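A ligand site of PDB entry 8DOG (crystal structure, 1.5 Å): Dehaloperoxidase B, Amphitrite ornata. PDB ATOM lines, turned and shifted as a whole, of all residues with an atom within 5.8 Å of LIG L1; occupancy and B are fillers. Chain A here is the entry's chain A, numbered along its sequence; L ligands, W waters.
An iron atom (FE1) of LIG L1 is bound by a ring nitrogen (NE2) of His 89 (2.1 Å). An oxygen (O3) of LIG L1 is in hydrogen-bond range of a ring nitrogen (ND1) of His 55 (2.6 Å). The side-chain amide nitrogen of Gln 88 sits at hydrogen-bond distance from an oxygen (O2) of LIG L1 (3.2 Å). The side-chain hydroxyl (OH) of Tyr 38 is in hydrogen-bond range of an oxygen (O2) of LG2 L2.
An oxygen (O4) of LIG L1 lies within hydrogen-bond range of an oxygen (O2) of LG2 L2 (2.5 Å).
SD of Met 86 lies close to ND1 of His 89. A ring nitrogen (ND1) of His 89 sits at hydrogen-bond distance from the backbone carbonyl oxygen of Leu 83 (2.8 Å). The side-chain amino group (NZ) of Lys 58 lies within salt-bridge range of the side-chain carboxylate (OD2) of Asp 54, at 3.0 Å. The side-chain carboxylate of Glu 31 sits at hydrogen-bond distance from the side-chain amide nitrogen of Asn 96 (2.7 Å). O of Glu 31 sits at hydrogen-bond distance from ND2 of Asn 34, 3.1 Å away.
Phe 24 touches LIG L1 (CZ to C26, 3.7 Å). Glu 31 touches LIG L1 (OE2 to C26, 3.5 Å). Asn 34 touches LIG L1. Phe 35 touches LIG L1. Lys 58 touches LIG L1. CG2 of Val 59 touches C8 of LIG L1, 3.5 Å away. Met 63 touches LIG L1 (N to C17, 3.5 Å). CD2 of Leu 83 touches C14 of LIG L1, 3.8 Å away. Met 86 touches LIG L1. CD1 of Leu 92 touches C23 of LIG L1, at 3.5 Å. Asn 96 touches LIG L1 (O to C24, 3.5 Å). Phe 97 touches LIG L1 (CE2 to C3, 3.2 Å). Leu 100 touches LIG L1 (CD2 to C24, 3.9 Å). CD2 of Leu 127 touches C19 of LIG L1 (3.8 Å). Hydrophobic or aromatic side chains within 4 Å of LIG L1: Phe 24, Phe 35, His 55, Val 59, Met 63, Leu 83, Met 86, His 89, Leu 92, Phe 97, Leu 100 and Leu 127.
Water W1 lies within hydrogen-bond range of O1 of LIG L1 (2.4 Å), OD2 of Asp 54 (2.8 Å) and NZ of Lys 58 (3.0 Å). Water W2 lies within hydrogen-bond range of the side-chain amide oxygen of Gln 88 (3.1 Å) and an oxygen (O2) of LIG L1 (3.3 Å).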
ATOM      1  N   PHE A  24     -27.804  15.903  21.227  1.00  0.00           N
ATOM      2  CA  PHE A  24     -26.642  15.684  22.111  1.00  0.00           C
ATOM      3  C   PHE A  24     -26.484  16.805  23.131  1.00  0.00           C
ATOM      4  O   PHE A  24     -26.310  16.478  24.322  1.00  0.00           O
ATOM      5  CB  PHE A  24     -25.442  15.503  21.190  1.00  0.00           C
ATOM      6  CG  PHE A  24     -24.114  15.534  21.898  1.00  0.00           C
ATOM      7  CD1 PHE A  24     -23.733  14.542  22.771  1.00  0.00           C
ATOM      8  CD2 PHE A  24     -23.212  16.573  21.663  1.00  0.00           C
ATOM      9  CE1 PHE A  24     -22.486  14.552  23.378  1.00  0.00           C
ATOM     10  CE2 PHE A  24     -21.955  16.570  22.245  1.00  0.00           C
ATOM     11  CZ  PHE A  24     -21.588  15.573  23.120  1.00  0.00           C
ATOM     12  N   GLU A  31     -21.652  19.062  28.117  1.00  0.00           N
ATOM     13  CA  GLU A  31     -20.803  18.963  26.899  1.00  0.00           C
ATOM     14  C   GLU A  31     -20.610  20.351  26.250  1.00  0.00           C
ATOM     15  O   GLU A  31     -19.680  20.519  25.447  1.00  0.00           O
ATOM     16  CB  GLU A  31     -21.429  17.932  25.949  1.00  0.00           C
ATOM     17  CG  GLU A  31     -21.323  16.507  26.520  1.00  0.00           C
ATOM     18  CD  GLU A  31     -19.885  15.997  26.621  1.00  0.00           C
ATOM     19  OE1 GLU A  31     -19.497  15.476  27.702  1.00  0.00           O
ATOM     20  OE2 GLU A  31     -19.170  16.089  25.642  1.00  0.00           O
ATOM     21  N   ASN A  34     -17.198  22.321  25.815  1.00  0.00           N
ATOM     22  CA  ASN A  34     -16.362  22.162  24.599  1.00  0.00           C
ATOM     23  C   ASN A  34     -16.788  23.139  23.505  1.00  0.00           C
ATOM     24  O   ASN A  34     -16.139  23.167  22.465  1.00  0.00           O
ATOM     25  CB  ASN A  34     -16.419  20.761  23.995  1.00  0.00           C
ATOM     26  CG  ASN A  34     -16.082  19.668  24.983  1.00  0.00           C
ATOM     27  OD1 ASN A  34     -14.924  19.576  25.341  1.00  0.00           O
ATOM     28  ND2 ASN A  34     -17.074  18.871  25.415  1.00  0.00           N
ATOM     29  N   PHE A  35     -17.923  23.850  23.710  1.00  0.00           N
ATOM     30  CA  PHE A  35     -18.579  24.672  22.666  1.00  0.00           C
ATOM     31  C   PHE A  35     -19.087  25.981  23.265  1.00  0.00           C
ATOM     32  O   PHE A  35     -20.267  26.225  23.281  1.00  0.00           O
ATOM     33  CB  PHE A  35     -19.764  23.922  22.057  1.00  0.00           C
ATOM     34  CG  PHE A  35     -19.416  22.577  21.536  1.00  0.00           C
ATOM     35  CD1 PHE A  35     -18.755  22.472  20.335  1.00  0.00           C
ATOM     36  CD2 PHE A  35     -19.690  21.426  22.265  1.00  0.00           C
ATOM     37  CE1 PHE A  35     -18.449  21.219  19.849  1.00  0.00           C
ATOM     38  CE2 PHE A  35     -19.319  20.187  21.789  1.00  0.00           C
ATOM     39  CZ  PHE A  35     -18.713  20.097  20.571  1.00  0.00           C
ATOM     40  N   TYR A  38     -21.727  28.411  21.974  1.00  0.00           N
ATOM     41  CA  TYR A  38     -23.139  27.913  21.862  1.00  0.00           C
ATOM     42  C   TYR A  38     -23.937  28.059  23.150  1.00  0.00           C
ATOM     43  O   TYR A  38     -25.148  27.714  23.169  1.00  0.00           O
ATOM     44  CB  TYR A  38     -23.185  26.491  21.324  1.00  0.00           C
ATOM     45  CG  TYR A  38     -22.494  26.295  20.007  1.00  0.00           C
ATOM     46  CD1 TYR A  38     -22.326  27.312  19.099  1.00  0.00           C
ATOM     47  CD2 TYR A  38     -22.030  25.038  19.654  1.00  0.00           C
ATOM     48  CE1 TYR A  38     -21.718  27.101  17.869  1.00  0.00           C
ATOM     49  CE2 TYR A  38     -21.384  24.819  18.446  1.00  0.00           C
ATOM     50  CZ  TYR A  38     -21.225  25.840  17.541  1.00  0.00           C
ATOM     51  OH  TYR A  38     -20.553  25.640  16.362  1.00  0.00           O
ATOM     52  N   ASP A  54     -22.233  25.591   9.700  1.00  0.00           N
ATOM     53  CA  ASP A  54     -21.041  25.192   8.917  1.00  0.00           C
ATOM     54  C   ASP A  54     -20.334  24.020   9.587  1.00  0.00           C
ATOM     55  O   ASP A  54     -20.057  23.005   8.922  1.00  0.00           O
ATOM     56  CB  ASP A  54     -20.051  26.339   8.756  1.00  0.00           C
ATOM     57  CG  ASP A  54     -18.925  25.999   7.770  1.00  0.00           C
ATOM     58  OD1 ASP A  54     -19.234  25.591   6.630  1.00  0.00           O
ATOM     59  OD2 ASP A  54     -17.727  26.187   8.098  1.00  0.00           O
ATOM     60  N   HIS A  55     -20.063  24.157  10.873  1.00  0.00           N
ATOM     61  CA  HIS A  55     -19.258  23.164  11.628  1.00  0.00           C
ATOM     62  C   HIS A  55     -20.090  21.887  11.744  1.00  0.00           C
ATOM     63  O   HIS A  55     -19.547  20.813  11.521  1.00  0.00           O
ATOM     64  CB  HIS A  55     -18.738  23.681  12.962  1.00  0.00           C
ATOM     65  CG  HIS A  55     -17.655  24.720  12.814  1.00  0.00           C
ATOM     66  ND1 HIS A  55     -16.533  24.714  13.600  1.00  0.00           N
ATOM     67  CD2 HIS A  55     -17.526  25.779  11.984  1.00  0.00           C
ATOM     68  CE1 HIS A  55     -15.754  25.727  13.281  1.00  0.00           C
ATOM     69  NE2 HIS A  55     -16.353  26.417  12.316  1.00  0.00           N
ATOM     70  N   LYS A  58     -19.882  20.029   8.484  1.00  0.00           N
ATOM     71  CA  LYS A  58     -18.556  19.454   8.161  1.00  0.00           C
ATOM     72  C   LYS A  58     -18.316  18.256   9.077  1.00  0.00           C
ATOM     73  O   LYS A  58     -17.759  17.242   8.614  1.00  0.00           O
ATOM     74  CB  LYS A  58     -17.544  20.568   8.248  1.00  0.00           C
ATOM     75  CG  LYS A  58     -17.560  21.486   7.028  1.00  0.00           C
ATOM     76  CD  LYS A  58     -16.686  22.651   7.226  1.00  0.00           C
ATOM     77  CE  LYS A  58     -16.589  23.490   5.969  1.00  0.00           C
ATOM     78  NZ  LYS A  58     -15.916  24.782   6.220  1.00  0.00           N
ATOM     79  N   VAL A  59     -18.703  18.313  10.327  1.00  0.00           N
ATOM     80  CA  VAL A  59     -18.557  17.179  11.253  1.00  0.00           C
ATOM     81  C   VAL A  59     -19.330  16.004  10.671  1.00  0.00           C
ATOM     82  O   VAL A  59     -18.811  14.884  10.590  1.00  0.00           O
ATOM     83  CB  VAL A  59     -19.018  17.504  12.681  1.00  0.00           C
ATOM     84  CG1 VAL A  59     -19.124  16.225  13.519  1.00  0.00           C
ATOM     85  CG2 VAL A  59     -18.111  18.526  13.333  1.00  0.00           C
ATOM     86  N   PHE A  60     -20.584  16.202  10.331  1.00  0.00           N
ATOM     87  CA  PHE A  60     -21.431  15.090   9.909  1.00  0.00           C
ATOM     88  C   PHE A  60     -21.008  14.544   8.553  1.00  0.00           C
ATOM     89  O   PHE A  60     -21.138  13.341   8.310  1.00  0.00           O
ATOM     90  CB  PHE A  60     -22.867  15.603   9.891  1.00  0.00           C
ATOM     91  CG  PHE A  60     -23.909  14.565  10.062  1.00  0.00           C
ATOM     92  CD1 PHE A  60     -24.155  14.032  11.332  1.00  0.00           C
ATOM     93  CD2 PHE A  60     -24.558  14.075   8.945  1.00  0.00           C
ATOM     94  CE1 PHE A  60     -25.081  13.015  11.452  1.00  0.00           C
ATOM     95  CE2 PHE A  60     -25.511  13.078   9.095  1.00  0.00           C
ATOM     96  CZ  PHE A  60     -25.726  12.534  10.336  1.00  0.00           C
ATOM     97  N   LEU A  62     -17.971  14.204   7.601  1.00  0.00           N
ATOM     98  CA  LEU A  62     -16.884  13.253   7.860  1.00  0.00           C
ATOM     99  C   LEU A  62     -17.427  12.074   8.628  1.00  0.00           C
ATOM    100  O   LEU A  62     -17.023  10.937   8.320  1.00  0.00           O
ATOM    101  CB  LEU A  62     -15.736  13.964   8.593  1.00  0.00           C
ATOM    102  CG  LEU A  62     -14.564  13.055   8.936  1.00  0.00           C
ATOM    103  CD1 LEU A  62     -13.933  12.339   7.734  1.00  0.00           C
ATOM    104  CD2 LEU A  62     -13.532  13.827   9.683  1.00  0.00           C
ATOM    105  N   MET A  63     -18.355  12.234   9.552  1.00  0.00           N
ATOM    106  CA  MET A  63     -18.905  11.104  10.300  1.00  0.00           C
ATOM    107  C   MET A  63     -19.459  10.093   9.256  1.00  0.00           C
ATOM    108  O   MET A  63     -19.331   8.855   9.473  1.00  0.00           O
ATOM    109  CB  MET A  63     -20.011  11.544  11.290  1.00  0.00           C
ATOM    110  CG  MET A  63     -20.463  10.424  12.175  1.00  0.00           C
ATOM    111  SD  MET A  63     -21.997  10.834  13.040  1.00  0.00           S
ATOM    112  CE  MET A  63     -21.493  12.231  14.049  1.00  0.00           C
ATOM    113  N   VAL A  66     -16.750   8.154   7.585  1.00  0.00           N
ATOM    114  CA  VAL A  66     -16.195   7.155   8.535  1.00  0.00           C
ATOM    115  C   VAL A  66     -17.122   5.936   8.587  1.00  0.00           C
ATOM    116  O   VAL A  66     -16.688   4.765   8.515  1.00  0.00           O
ATOM    117  CB  VAL A  66     -15.835   7.729   9.892  1.00  0.00           C
ATOM    118  CG1 VAL A  66     -15.398   6.670  10.866  1.00  0.00           C
ATOM    119  CG2 VAL A  66     -14.804   8.826   9.713  1.00  0.00           C
ATOM    120  N   LEU A  83      -9.251  11.082  13.753  1.00  0.00           N
ATOM    121  CA  LEU A  83     -10.118  11.686  14.797  1.00  0.00           C
ATOM    122  C   LEU A  83      -9.357  11.913  16.102  1.00  0.00           C
ATOM    123  O   LEU A  83      -9.598  12.926  16.738  1.00  0.00           O
ATOM    124  CB  LEU A  83     -11.333  10.807  15.032  1.00  0.00           C
ATOM    125  CG  LEU A  83     -12.264  10.765  13.846  1.00  0.00           C
ATOM    126  CD1 LEU A  83     -13.303   9.679  14.059  1.00  0.00           C
ATOM    127  CD2 LEU A  83     -12.923  12.123  13.552  1.00  0.00           C
ATOM    128  N   MET A  86      -6.504  15.033  15.242  1.00  0.00           N
ATOM    129  CA  MET A  86      -7.037  16.367  14.836  1.00  0.00           C
ATOM    130  C   MET A  86      -6.815  17.372  15.977  1.00  0.00           C
ATOM    131  O   MET A  86      -7.166  17.050  17.121  1.00  0.00           O
ATOM    132  CB  MET A  86      -8.541  16.265  14.565  1.00  0.00           C
ATOM    133  CG  MET A  86      -8.896  15.817  13.240  1.00  0.00           C
ATOM    134  SD  MET A  86     -10.697  15.521  13.275  1.00  0.00           S
ATOM    135  CE  MET A  86     -11.415  17.144  13.498  1.00  0.00           C
ATOM    136  N   GLN A  88      -8.369  19.943  16.687  1.00  0.00           N
ATOM    137  CA  GLN A  88      -9.664  20.408  17.243  1.00  0.00           C
ATOM    138  C   GLN A  88     -10.162  19.413  18.295  1.00  0.00           C
ATOM    139  O   GLN A  88     -11.069  19.787  19.056  1.00  0.00           O
ATOM    140  CB  GLN A  88     -10.683  20.693  16.135  1.00  0.00           C
ATOM    141  CG  GLN A  88     -10.436  22.029  15.434  1.00  0.00           C
ATOM    142  CD  GLN A  88     -11.064  22.112  14.064  1.00  0.00           C
ATOM    143  OE1 GLN A  88     -10.761  21.289  13.211  1.00  0.00           O
ATOM    144  NE2 GLN A  88     -11.917  23.101  13.826  1.00  0.00           N
ATOM    145  N   HIS A  89      -9.612  18.194  18.315  1.00  0.00           N
ATOM    146  CA  HIS A  89      -9.966  17.143  19.286  1.00  0.00           C
ATOM    147  C   HIS A  89      -8.962  16.981  20.440  1.00  0.00           C
ATOM    148  O   HIS A  89      -9.134  16.018  21.255  1.00  0.00           O
ATOM    149  CB  HIS A  89     -10.161  15.815  18.557  1.00  0.00           C
ATOM    150  CG  HIS A  89     -11.395  15.798  17.728  1.00  0.00           C
ATOM    151  ND1 HIS A  89     -11.667  14.770  16.841  1.00  0.00           N
ATOM    152  CD2 HIS A  89     -12.466  16.650  17.635  1.00  0.00           C
ATOM    153  CE1 HIS A  89     -12.790  15.013  16.224  1.00  0.00           C
ATOM    154  NE2 HIS A  89     -13.306  16.143  16.658  1.00  0.00           N
ATOM    155  N   LEU A  92     -10.339  16.151  24.065  1.00  0.00           N
ATOM    156  CA  LEU A  92     -11.467  15.198  24.206  1.00  0.00           C
ATOM    157  C   LEU A  92     -10.999  13.857  24.750  1.00  0.00           C
ATOM    158  O   LEU A  92      -9.787  13.488  24.632  1.00  0.00           O
ATOM    159  CB  LEU A  92     -12.096  15.007  22.839  1.00  0.00           C
ATOM    160  CG  LEU A  92     -12.599  16.276  22.155  1.00  0.00           C
ATOM    161  CD1 LEU A  92     -13.318  15.920  20.870  1.00  0.00           C
ATOM    162  CD2 LEU A  92     -13.528  17.097  23.053  1.00  0.00           C
ATOM    163  N   ASN A  96     -16.771  11.627  25.486  1.00  0.00           N
ATOM    164  CA  ASN A  96     -17.443  12.667  24.660  1.00  0.00           C
ATOM    165  C   ASN A  96     -18.098  11.966  23.476  1.00  0.00           C
ATOM    166  O   ASN A  96     -19.235  12.281  23.101  1.00  0.00           O
ATOM    167  CB  ASN A  96     -16.437  13.672  24.169  1.00  0.00           C
ATOM    168  CG  ASN A  96     -15.781  14.477  25.280  1.00  0.00           C
ATOM    169  OD1 ASN A  96     -14.564  14.391  25.523  1.00  0.00           O
ATOM    170  ND2 ASN A  96     -16.562  15.310  25.932  1.00  0.00           N
ATOM    171  N   PHE A  97     -17.388  11.006  22.877  1.00  0.00           N
ATOM    172  CA  PHE A  97     -17.895  10.238  21.723  1.00  0.00           C
ATOM    173  C   PHE A  97     -18.946   9.247  22.153  1.00  0.00           C
ATOM    174  O   PHE A  97     -19.917   9.085  21.399  1.00  0.00           O
ATOM    175  CB  PHE A  97     -16.734   9.533  20.964  1.00  0.00           C
ATOM    176  CG  PHE A  97     -15.819  10.508  20.269  1.00  0.00           C
ATOM    177  CD1 PHE A  97     -14.824  11.191  20.977  1.00  0.00           C
ATOM    178  CD2 PHE A  97     -15.930  10.724  18.911  1.00  0.00           C
ATOM    179  CE1 PHE A  97     -14.029  12.116  20.328  1.00  0.00           C
ATOM    180  CE2 PHE A  97     -15.117  11.643  18.257  1.00  0.00           C
ATOM    181  CZ  PHE A  97     -14.162  12.318  18.992  1.00  0.00           C
ATOM    182  N   LEU A 100     -22.124  11.263  22.472  1.00  0.00           N
ATOM    183  CA  LEU A 100     -22.647  11.591  21.156  1.00  0.00           C
ATOM    184  C   LEU A 100     -23.422  10.417  20.563  1.00  0.00           C
ATOM    185  O   LEU A 100     -24.528  10.654  20.055  1.00  0.00           O
ATOM    186  CB  LEU A 100     -21.534  12.082  20.250  1.00  0.00           C
ATOM    187  CG  LEU A 100     -21.908  12.345  18.798  1.00  0.00           C
ATOM    188  CD1 LEU A 100     -22.999  13.393  18.703  1.00  0.00           C
ATOM    189  CD2 LEU A 100     -20.688  12.716  17.973  1.00  0.00           C
ATOM    190  N   PHE A 101     -22.868   9.216  20.606  1.00  0.00           N
ATOM    191  CA  PHE A 101     -23.546   8.109  19.902  1.00  0.00           C
ATOM    192  C   PHE A 101     -24.779   7.656  20.726  1.00  0.00           C
ATOM    193  O   PHE A 101     -25.721   7.177  20.065  1.00  0.00           O
ATOM    194  CB  PHE A 101     -22.538   7.024  19.480  1.00  0.00           C
ATOM    195  CG  PHE A 101     -21.856   7.463  18.227  1.00  0.00           C
ATOM    196  CD1 PHE A 101     -22.397   7.210  16.986  1.00  0.00           C
ATOM    197  CD2 PHE A 101     -20.690   8.204  18.299  1.00  0.00           C
ATOM    198  CE1 PHE A 101     -21.848   7.742  15.840  1.00  0.00           C
ATOM    199  CE2 PHE A 101     -20.125   8.695  17.153  1.00  0.00           C
ATOM    200  CZ  PHE A 101     -20.720   8.487  15.931  1.00  0.00           C
ATOM    201  N   LEU A 127     -16.429   2.605  17.411  1.00  0.00           N
ATOM    202  CA  LEU A 127     -15.612   3.813  17.183  1.00  0.00           C
ATOM    203  C   LEU A 127     -14.922   4.191  18.489  1.00  0.00           C
ATOM    204  O   LEU A 127     -13.731   4.479  18.484  1.00  0.00           O
ATOM    205  CB  LEU A 127     -16.496   4.947  16.697  1.00  0.00           C
ATOM    206  CG  LEU A 127     -15.757   6.270  16.537  1.00  0.00           C
ATOM    207  CD1 LEU A 127     -14.639   6.190  15.495  1.00  0.00           C
ATOM    208  CD2 LEU A 127     -16.726   7.395  16.202  1.00  0.00           C
HETATM  209  C1  LIG L   1     -14.266  20.071  15.117  1.00  0.00           C
HETATM  210  C2  LIG L   1     -15.356  15.761  13.048  1.00  0.00           C
HETATM  211  C3  LIG L   1     -16.949  14.142  17.352  1.00  0.00           C
HETATM  212  C4  LIG L   1     -15.652  18.362  19.414  1.00  0.00           C
HETATM  213  C5  LIG L   1     -14.488  19.049  14.159  1.00  0.00           C
HETATM  214  C6  LIG L   1     -14.304  19.165  12.722  1.00  0.00           C
HETATM  215  C7  LIG L   1     -14.620  17.910  12.135  1.00  0.00           C
HETATM  216  C8  LIG L   1     -14.950  17.100  13.238  1.00  0.00           C
HETATM  217  C9  LIG L   1     -14.549  17.596  10.654  1.00  0.00           C
HETATM  218  C10 LIG L   1     -13.931  20.447  11.997  1.00  0.00           C
HETATM  219  C11 LIG L   1     -15.165  21.326  11.796  1.00  0.00           C
HETATM  220  C12 LIG L   1     -14.924  22.643  11.104  1.00  0.00           C
HETATM  221  O1  LIG L   1     -15.805  23.263  10.473  1.00  0.00           O
HETATM  222  O2  LIG L   1     -13.818  23.234  11.305  1.00  0.00           O
HETATM  223  C13 LIG L   1     -15.858  14.960  14.043  1.00  0.00           C
HETATM  224  C14 LIG L   1     -16.393  13.608  13.773  1.00  0.00           C
HETATM  225  C15 LIG L   1     -16.878  13.198  14.970  1.00  0.00           C
HETATM  226  C16 LIG L   1     -16.610  14.213  16.021  1.00  0.00           C
HETATM  227  C17 LIG L   1     -16.527  12.922  12.433  1.00  0.00           C
HETATM  228  C18 LIG L   1     -17.563  11.959  15.394  1.00  0.00           C
HETATM  229  C19 LIG L   1     -17.356  10.798  14.738  1.00  0.00           C
HETATM  230  C20 LIG L   1     -16.761  15.185  18.238  1.00  0.00           C
HETATM  231  C21 LIG L   1     -17.203  15.147  19.596  1.00  0.00           C
HETATM  232  C22 LIG L   1     -16.833  16.345  20.183  1.00  0.00           C
HETATM  233  C23 LIG L   1     -16.191  17.098  19.162  1.00  0.00           C
HETATM  234  C24 LIG L   1     -17.850  13.942  20.309  1.00  0.00           C
HETATM  235  C25 LIG L   1     -17.052  16.790  21.541  1.00  0.00           C
HETATM  236  C26 LIG L   1     -18.043  16.342  22.337  1.00  0.00           C
HETATM  237  C27 LIG L   1     -15.100  19.093  18.345  1.00  0.00           C
HETATM  238  C28 LIG L   1     -14.643  20.479  18.606  1.00  0.00           C
HETATM  239  C29 LIG L   1     -14.274  20.963  17.405  1.00  0.00           C
HETATM  240  C30 LIG L   1     -14.563  19.929  16.427  1.00  0.00           C
HETATM  241  C31 LIG L   1     -14.612  21.155  19.955  1.00  0.00           C
HETATM  242  C32 LIG L   1     -13.666  22.309  17.026  1.00  0.00           C
HETATM  243  C33 LIG L   1     -14.474  23.482  17.434  1.00  0.00           C
HETATM  244  C34 LIG L   1     -15.644  23.586  16.531  1.00  0.00           C
HETATM  245  O3  LIG L   1     -15.608  23.126  15.384  1.00  0.00           O
HETATM  246  O4  LIG L   1     -16.712  24.191  16.973  1.00  0.00           O
HETATM  247  N1  LIG L   1     -14.904  17.757  14.467  1.00  0.00           N
HETATM  248  N2  LIG L   1     -15.983  15.245  15.374  1.00  0.00           N
HETATM  249  N3  LIG L   1     -16.175  16.364  17.989  1.00  0.00           N
HETATM  250  N4  LIG L   1     -14.965  18.790  17.039  1.00  0.00           N
HETATM  251 FE1  LIG L   1     -15.251  16.959  16.249  1.00  0.00          FE
HETATM  252  C1  LG2 L   2     -19.806  17.230  18.193  1.00  0.00           C
HETATM  253  C2  LG2 L   2     -22.812  17.303  14.209  1.00  0.00           C
HETATM  254  C3  LG2 L   2     -23.210  15.844  16.027  1.00  0.00           C
HETATM  255  C4  LG2 L   2     -18.178  21.120  16.366  1.00  0.00           C
HETATM  256  C5  LG2 L   2     -20.538  21.573  16.288  1.00  0.00           C
HETATM  257  C6  LG2 L   2     -21.652  17.754  14.851  1.00  0.00           C
HETATM  258  C7  LG2 L   2     -22.089  16.321  16.693  1.00  0.00           C
HETATM  259  C8  LG2 L   2     -18.431  19.768  16.546  1.00  0.00           C
HETATM  260  C9  LG2 L   2     -20.782  20.213  16.516  1.00  0.00           C
HETATM  261  C10 LG2 L   2     -23.571  16.303  14.774  1.00  0.00           C
HETATM  262  C11 LG2 L   2     -19.231  22.029  16.289  1.00  0.00           C
HETATM  263  C12 LG2 L   2     -21.276  17.298  16.112  1.00  0.00           C
HETATM  264  C13 LG2 L   2     -19.750  19.277  16.634  1.00  0.00           C
HETATM  265  C14 LG2 L   2     -19.995  17.782  16.777  1.00  0.00           C
HETATM  266  O1  LG2 L   2     -24.697  15.872  14.108  1.00  0.00           O
HETATM  267  O2  LG2 L   2     -18.968  23.359  16.175  1.00  0.00           O
HETATM  268  O   HOH W   1     -15.306  25.266   9.168  1.00  0.00           O
HETATM  269  O   HOH W   2     -11.129  21.685  10.144  1.00  0.00           O
HETATM  270  O   HOH W   3     -16.898  25.752  19.034  1.00  0.00           O
